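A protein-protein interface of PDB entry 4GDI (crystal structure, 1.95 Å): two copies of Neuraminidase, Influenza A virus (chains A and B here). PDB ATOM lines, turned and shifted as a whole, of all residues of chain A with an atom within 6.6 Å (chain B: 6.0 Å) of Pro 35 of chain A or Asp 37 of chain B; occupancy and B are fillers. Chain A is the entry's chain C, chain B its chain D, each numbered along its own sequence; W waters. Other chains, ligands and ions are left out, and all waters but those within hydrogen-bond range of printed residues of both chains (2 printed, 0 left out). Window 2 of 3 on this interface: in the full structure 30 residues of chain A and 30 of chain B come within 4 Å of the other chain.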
ATOM      1  N   TRP A  30       3.473   1.568  17.028  1.00  0.00           N
ATOM      2  CA  TRP A  30       2.323   0.807  16.575  1.00  0.00           C
ATOM      3  C   TRP A  30       2.769  -0.414  15.783  1.00  0.00           C
ATOM      4  O   TRP A  30       3.856  -0.431  15.198  1.00  0.00           O
ATOM      5  CB  TRP A  30       1.417   1.671  15.700  1.00  0.00           C
ATOM      6  CG  TRP A  30       0.976   2.971  16.321  1.00  0.00           C
ATOM      7  CD1 TRP A  30       0.843   4.168  15.687  1.00  0.00           C
ATOM      8  CD2 TRP A  30       0.607   3.200  17.691  1.00  0.00           C
ATOM      9  NE1 TRP A  30       0.413   5.130  16.572  1.00  0.00           N
ATOM     10  CE2 TRP A  30       0.258   4.561  17.807  1.00  0.00           C
ATOM     11  CE3 TRP A  30       0.538   2.390  18.828  1.00  0.00           C
ATOM     12  CZ2 TRP A  30      -0.146   5.131  19.016  1.00  0.00           C
ATOM     13  CZ3 TRP A  30       0.130   2.957  20.029  1.00  0.00           C
ATOM     14  CH2 TRP A  30      -0.204   4.315  20.112  1.00  0.00           C
ATOM     15  N   GLU A  33      -0.639  -4.277  16.244  1.00  0.00           N
ATOM     16  CA  GLU A  33      -1.952  -3.649  16.384  1.00  0.00           C
ATOM     17  C   GLU A  33      -1.841  -2.134  16.578  1.00  0.00           C
ATOM     18  O   GLU A  33      -0.786  -1.612  16.941  1.00  0.00           O
ATOM     19  CB  GLU A  33      -2.738  -4.278  17.539  1.00  0.00           C
ATOM     20  CG  GLU A  33      -3.014  -5.770  17.355  1.00  0.00           C
ATOM     21  CD  GLU A  33      -3.842  -6.358  18.481  1.00  0.00           C
ATOM     22  OE1 GLU A  33      -3.511  -6.124  19.668  1.00  0.00           O
ATOM     23  OE2 GLU A  33      -4.831  -7.057  18.176  1.00  0.00           O
ATOM     24  N   LEU A  34      -2.938  -1.433  16.334  1.00  0.00           N
ATOM     25  CA  LEU A  34      -2.971  -0.001  16.572  1.00  0.00           C
ATOM     26  C   LEU A  34      -4.319   0.375  17.150  1.00  0.00           C
ATOM     27  O   LEU A  34      -5.309  -0.336  16.943  1.00  0.00           O
ATOM     28  CB  LEU A  34      -2.647   0.783  15.290  1.00  0.00           C
ATOM     29  CG  LEU A  34      -3.607   0.761  14.103  1.00  0.00           C
ATOM     30  CD1 LEU A  34      -2.976   1.526  12.947  1.00  0.00           C
ATOM     31  CD2 LEU A  34      -3.966  -0.652  13.680  1.00  0.00           C
ATOM     32  N   PRO A  35      -4.360   1.465  17.927  1.00  0.00           N
ATOM     33  CA  PRO A  35      -5.654   1.869  18.470  1.00  0.00           C
ATOM     34  C   PRO A  35      -6.553   2.340  17.348  1.00  0.00           C
ATOM     35  O   PRO A  35      -6.061   2.637  16.258  1.00  0.00           O
ATOM     36  CB  PRO A  35      -5.299   3.041  19.401  1.00  0.00           C
ATOM     37  CG  PRO A  35      -4.077   3.603  18.841  1.00  0.00           C
ATOM     38  CD  PRO A  35      -3.297   2.422  18.283  1.00  0.00           C
ATOM     39  N   GLY A  36      -7.850   2.403  17.612  1.00  0.00           N
ATOM     40  CA  GLY A  36      -8.793   2.925  16.649  1.00  0.00           C
ATOM     41  C   GLY A  36      -8.730   4.435  16.604  1.00  0.00           C
ATOM     42  O   GLY A  36      -8.186   5.069  17.507  1.00  0.00           O
ATOM     43  N   ASP A  37      -9.264   5.001  15.529  1.00  0.00           N
ATOM     44  CA  ASP A  37      -9.359   6.451  15.365  1.00  0.00           C
ATOM     45  C   ASP A  37      -8.015   7.136  15.090  1.00  0.00           C
ATOM     46  O   ASP A  37      -7.911   8.355  15.216  1.00  0.00           O
ATOM     47  CB  ASP A  37     -10.036   7.087  16.586  1.00  0.00           C
ATOM     48  CG  ASP A  37     -11.470   6.599  16.785  1.00  0.00           C
ATOM     49  OD1 ASP A  37     -12.106   6.170  15.799  1.00  0.00           O
ATOM     50  OD2 ASP A  37     -11.963   6.649  17.933  1.00  0.00           O
ATOM     51  N   LEU A  38      -6.991   6.368  14.721  1.00  0.00           N
ATOM     52  CA  LEU A  38      -5.753   6.963  14.236  1.00  0.00           C
ATOM     53  C   LEU A  38      -5.934   7.328  12.770  1.00  0.00           C
ATOM     54  O   LEU A  38      -6.491   6.559  11.988  1.00  0.00           O
ATOM     55  CB  LEU A  38      -4.572   6.005  14.349  1.00  0.00           C
ATOM     56  CG  LEU A  38      -3.846   5.814  15.679  1.00  0.00           C
ATOM     57  CD1 LEU A  38      -2.604   4.968  15.428  1.00  0.00           C
ATOM     58  CD2 LEU A  38      -3.473   7.136  16.325  1.00  0.00           C
ATOM     59  N   SER A  63      -8.213   4.143  11.269  1.00  0.00           N
ATOM     60  CA  SER A  63      -8.222   2.786  11.805  1.00  0.00           C
ATOM     61  C   SER A  63      -9.501   2.514  12.606  1.00  0.00           C
ATOM     62  O   SER A  63     -10.064   3.412  13.222  1.00  0.00           O
ATOM     63  CB  SER A  63      -7.008   2.571  12.694  1.00  0.00           C
ATOM     64  OG  SER A  63      -7.104   3.376  13.852  1.00  0.00           O
ATOM     65  N   ALA A  64      -9.952   1.266  12.589  1.00  0.00           N
ATOM     66  CA  ALA A  64     -11.110   0.843  13.373  1.00  0.00           C
ATOM     67  C   ALA A  64     -11.006  -0.657  13.611  1.00  0.00           C
ATOM     68  O   ALA A  64     -11.146  -1.441  12.676  1.00  0.00           O
ATOM     69  CB  ALA A  64     -12.411   1.171  12.642  1.00  0.00           C
ATOM     70  N   ASN A  65     -10.747  -1.048  14.857  1.00  0.00           N
ATOM     71  CA  ASN A  65     -10.598  -2.458  15.212  1.00  0.00           C
ATOM     72  C   ASN A  65      -9.608  -3.177  14.297  1.00  0.00           C
ATOM     73  O   ASN A  65      -9.898  -4.253  13.768  1.00  0.00           O
ATOM     74  CB  ASN A  65     -11.954  -3.168  15.186  1.00  0.00           C
ATOM     75  CG  ASN A  65     -12.949  -2.558  16.156  1.00  0.00           C
ATOM     76  OD1 ASN A  65     -12.774  -2.634  17.373  1.00  0.00           O
ATOM     77  ND2 ASN A  65     -14.005  -1.952  15.620  1.00  0.00           N
ATOM     78  N   GLN A  66      -8.447  -2.553  14.111  1.00  0.00           N
ATOM     79  CA  GLN A  66      -7.317  -3.145  13.392  1.00  0.00           C
ATOM     80  C   GLN A  66      -7.461  -3.092  11.875  1.00  0.00           C
ATOM     81  O   GLN A  66      -6.489  -3.327  11.155  1.00  0.00           O
ATOM     82  CB  GLN A  66      -7.053  -4.588  13.855  1.00  0.00           C
ATOM     83  CG  GLN A  66      -6.726  -4.704  15.336  1.00  0.00           C
ATOM     84  CD  GLN A  66      -5.804  -3.587  15.840  1.00  0.00           C
ATOM     85  OE1 GLN A  66      -4.803  -3.251  15.201  1.00  0.00           O
ATOM     86  NE2 GLN A  66      -6.138  -3.019  16.999  1.00  0.00           N
ATOM     87  N   ALA A  87       0.104  11.456  18.940  1.00  0.00           N
ATOM     88  CA  ALA A  87      -0.362  10.563  17.897  1.00  0.00           C
ATOM     89  C   ALA A  87      -1.433  11.298  17.095  1.00  0.00           C
ATOM     90  O   ALA A  87      -2.152  12.146  17.630  1.00  0.00           O
ATOM     91  CB  ALA A  87      -0.928   9.286  18.496  1.00  0.00           C
ATOM     92  N   PRO B  35     -10.437   2.260  31.289  1.00  0.00           N
ATOM     93  CA  PRO B  35     -10.920   2.659  29.965  1.00  0.00           C
ATOM     94  C   PRO B  35      -9.937   2.307  28.854  1.00  0.00           C
ATOM     95  O   PRO B  35      -8.765   2.073  29.133  1.00  0.00           O
ATOM     96  CB  PRO B  35     -11.062   4.179  30.086  1.00  0.00           C
ATOM     97  CG  PRO B  35     -10.171   4.565  31.160  1.00  0.00           C
ATOM     98  CD  PRO B  35     -10.112   3.423  32.129  1.00  0.00           C
ATOM     99  N   GLY B  36     -10.404   2.282  27.612  1.00  0.00           N
ATOM    100  CA  GLY B  36      -9.534   1.986  26.490  1.00  0.00           C
ATOM    101  C   GLY B  36      -8.633   3.159  26.151  1.00  0.00           C
ATOM    102  O   GLY B  36      -8.908   4.294  26.528  1.00  0.00           O
ATOM    103  N   ASP B  37      -7.538   2.877  25.454  1.00  0.00           N
ATOM    104  CA  ASP B  37      -6.658   3.919  24.940  1.00  0.00           C
ATOM    105  C   ASP B  37      -5.959   4.700  26.056  1.00  0.00           C
ATOM    106  O   ASP B  37      -5.627   5.869  25.889  1.00  0.00           O
ATOM    107  CB  ASP B  37      -7.454   4.859  24.030  1.00  0.00           C
ATOM    108  CG  ASP B  37      -8.113   4.122  22.869  1.00  0.00           C
ATOM    109  OD1 ASP B  37      -7.401   3.378  22.157  1.00  0.00           O
ATOM    110  OD2 ASP B  37      -9.341   4.268  22.681  1.00  0.00           O
ATOM    111  N   LEU B  38      -5.750   4.041  27.195  1.00  0.00           N
ATOM    112  CA  LEU B  38      -4.913   4.582  28.256  1.00  0.00           C
ATOM    113  C   LEU B  38      -3.483   4.140  28.023  1.00  0.00           C
ATOM    114  O   LEU B  38      -3.225   2.971  27.713  1.00  0.00           O
ATOM    115  CB  LEU B  38      -5.369   4.099  29.640  1.00  0.00           C
ATOM    116  CG  LEU B  38      -6.448   4.898  30.385  1.00  0.00           C
ATOM    117  CD1 LEU B  38      -5.822   5.817  31.418  1.00  0.00           C
ATOM    118  CD2 LEU B  38      -7.284   5.701  29.418  1.00  0.00           C
ATOM    119  N   ILE B  39      -2.560   5.081  28.165  1.00  0.00           N
ATOM    120  CA  ILE B  39      -1.140   4.765  28.168  1.00  0.00           C
ATOM    121  C   ILE B  39      -0.758   4.285  29.564  1.00  0.00           C
ATOM    122  O   ILE B  39      -0.902   5.018  30.546  1.00  0.00           O
ATOM    123  CB  ILE B  39      -0.297   5.984  27.786  1.00  0.00           C
ATOM    124  CG1 ILE B  39      -0.839   6.596  26.492  1.00  0.00           C
ATOM    125  CG2 ILE B  39       1.176   5.580  27.641  1.00  0.00           C
ATOM    126  CD1 ILE B  39      -0.147   7.877  26.068  1.00  0.00           C
ATOM    127  N   LEU B  62      -0.524   0.253  25.808  1.00  0.00           N
ATOM    128  CA  LEU B  62      -1.810   0.905  25.586  1.00  0.00           C
ATOM    129  C   LEU B  62      -2.946  -0.067  25.872  1.00  0.00           C
ATOM    130  O   LEU B  62      -2.919  -1.215  25.412  1.00  0.00           O
ATOM    131  CB  LEU B  62      -1.903   1.398  24.138  1.00  0.00           C
ATOM    132  CG  LEU B  62      -2.863   2.569  23.882  1.00  0.00           C
ATOM    133  CD1 LEU B  62      -2.459   3.777  24.698  1.00  0.00           C
ATOM    134  CD2 LEU B  62      -2.915   2.942  22.409  1.00  0.00           C
ATOM    135  N   SER B  63      -3.938   0.381  26.639  1.00  0.00           N
ATOM    136  CA  SER B  63      -5.080  -0.464  26.969  1.00  0.00           C
ATOM    137  C   SER B  63      -6.061  -0.525  25.799  1.00  0.00           C
ATOM    138  O   SER B  63      -6.166   0.414  25.008  1.00  0.00           O
ATOM    139  CB  SER B  63      -5.795   0.046  28.228  1.00  0.00           C
ATOM    140  OG  SER B  63      -6.483   1.262  27.981  1.00  0.00           O
ATOM    141  N   ALA B  64      -6.772  -1.643  25.701  1.00  0.00           N
ATOM    142  CA  ALA B  64      -7.779  -1.845  24.668  1.00  0.00           C
ATOM    143  C   ALA B  64      -8.708  -2.972  25.110  1.00  0.00           C
ATOM    144  O   ALA B  64      -8.275  -4.122  25.267  1.00  0.00           O
ATOM    145  CB  ALA B  64      -7.120  -2.190  23.337  1.00  0.00           C
ATOM    146  N   LEU B  69      -2.991  -3.796  24.015  1.00  0.00           N
ATOM    147  CA  LEU B  69      -2.829  -3.762  22.578  1.00  0.00           C
ATOM    148  C   LEU B  69      -1.453  -4.340  22.265  1.00  0.00           C
ATOM    149  O   LEU B  69      -0.488  -4.100  22.998  1.00  0.00           O
ATOM    150  CB  LEU B  69      -2.940  -2.328  22.070  1.00  0.00           C
ATOM    151  CG  LEU B  69      -3.402  -2.123  20.629  1.00  0.00           C
ATOM    152  CD1 LEU B  69      -4.766  -2.758  20.405  1.00  0.00           C
ATOM    153  CD2 LEU B  69      -3.437  -0.633  20.310  1.00  0.00           C
ATOM    154  N   THR B  71       1.702  -4.128  20.753  1.00  0.00           N
ATOM    155  CA  THR B  71       2.557  -3.118  20.135  1.00  0.00           C
ATOM    156  C   THR B  71       3.978  -3.315  20.607  1.00  0.00           C
ATOM    157  O   THR B  71       4.235  -4.195  21.422  1.00  0.00           O
ATOM    158  CB  THR B  71       2.146  -1.696  20.548  1.00  0.00           C
ATOM    159  OG1 THR B  71       2.483  -1.489  21.925  1.00  0.00           O
ATOM    160  CG2 THR B  71       0.649  -1.476  20.343  1.00  0.00           C
ATOM    161  N   SER B  88      -3.905   9.499  31.363  1.00  0.00           N
ATOM    162  CA  SER B  88      -2.955   9.441  30.266  1.00  0.00           C
ATOM    163  C   SER B  88      -3.547   8.747  29.049  1.00  0.00           C
ATOM    164  O   SER B  88      -3.614   7.527  28.981  1.00  0.00           O
ATOM    165  CB  SER B  88      -1.685   8.717  30.693  1.00  0.00           C
ATOM    166  OG  SER B  88      -0.990   9.467  31.666  1.00  0.00           O
ATOM    167  N   THR B  89      -3.956   9.552  28.085  1.00  0.00           N
ATOM    168  CA  THR B  89      -4.489   9.052  26.832  1.00  0.00           C
ATOM    169  C   THR B  89      -3.669   9.645  25.705  1.00  0.00           C
ATOM    170  O   THR B  89      -2.884  10.580  25.918  1.00  0.00           O
ATOM    171  CB  THR B  89      -5.962   9.468  26.665  1.00  0.00           C
ATOM    172  OG1 THR B  89      -6.060  10.889  26.454  1.00  0.00           O
ATOM    173  CG2 THR B  89      -6.746   9.089  27.897  1.00  0.00           C
ATOM    174  N   LEU B  90      -3.856   9.117  24.503  1.00  0.00           N
ATOM    175  CA  LEU B  90      -3.174   9.650  23.328  1.00  0.00           C
ATOM    176  C   LEU B  90      -3.536  11.119  23.110  1.00  0.00           C
ATOM    177  O   LEU B  90      -2.821  11.858  22.430  1.00  0.00           O
ATOM    178  CB  LEU B  90      -3.563   8.851  22.095  1.00  0.00           C
ATOM    179  CG  LEU B  90      -3.301   7.351  22.193  1.00  0.00           C
ATOM    180  CD1 LEU B  90      -4.170   6.609  21.188  1.00  0.00           C
ATOM    181  CD2 LEU B  90      -1.836   7.056  21.968  1.00  0.00           C
HETATM  182  O   HOH W   1      -8.465   0.691  20.425  1.00  0.00           O
HETATM  183  O   HOH W   2      -0.565  10.918  21.580  1.00  0.00           O
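O of Leu 34 of chain A lies within hydrogen-bond range of NE2 of Gln 66 of chain A (2.8 Å). N of Asp 37 of chain B sits at hydrogen-bond distance from O of Ser 63 of chain B (2.9 Å). The backbone carbonyl oxygen (O) of Pro 35 of chain A is in hydrogen-bond range of the side-chain hydroxyl (OG) of Ser 63 of chain A (2.7 Å). N of Leu 69 of chain B lies within hydrogen-bond range of O of Leu 62 of chain B (2.9 Å).
Among the printed residues, merely in contact across the chains: Trp 30 of chain A with Leu 62 of chain B, Trp 30 of chain A with Leu 90 of chain B, Glu 33 of chain A with Leu 69 of chain B, Glu 33 of chain A with Thr 71 of chain B, Leu 34 of chain A with Leu 69 of chain B, Pro 35 of chain A with Asp 37 of chain B, Pro 35 of chain A with Leu 62 of chain B, Pro 35 of chain A with Leu 69 of chain B, Pro 35 of chain A with Leu 90 of chain B and Gln 66 of chain A with Leu 69 of chain B.
Of the printed residues of chain B, Pro 35 of chain A touches Asp 37 (3.5 Å), Leu 62 (3.8 Å), Leu 69 (3.3 Å) and Leu 90 (3.8 Å). Of the printed residues of chain A, Asp 37 of chain B touches Pro 35. Of the printed residues of chain A, Thr 71 of chain B touches Glu 33. Printed residues of chain A within 4 Å of Leu 69 of chain B: Glu 33 (3.7 Å), Leu 34 (3.4 Å), Pro 35 (3.3 Å) and Gln 66 (3.7 Å). Leu 38 of chain B touches none of the printed residues of chain A. The nearest printed residue of chain A that does not touch Thr 71 of chain B is Trp 30 of chain A (4.2 Å).
Of the 12 printed residues of chain A, 5 touch a printed residue of chain B. Among the printed residues, 10 pairs touch across the chains. Among the printed residues, no Asp or Glu carboxylate lies within 4 Å of a Lys or Arg side-chain nitrogen of the other chain.
Pro 35 of chain A touches Asp 37 of chain B, but with the chains exchanged Asp 37 of chain A does not touch Pro 35 of chain B (11.9 Å). Positions printed for both chains: 35, 36, 37, 38, 63 and 64. Of the 10 pairs that touch across the chains among the printed residues, none has its exchanged pair printed and touching as well.
Water W2 lies within hydrogen-bond range of the backbone carbonyl oxygen (O) of Leu 90 of chain B (2.6 Å) and the backbone NH (N) of Ala 87 of chain A (2.8 Å). Water W1 lies within hydrogen-bond range of N of Gly 36 of chain A (3.3 Å) and OD1 of Asp 37 of chain B (3.4 Å).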
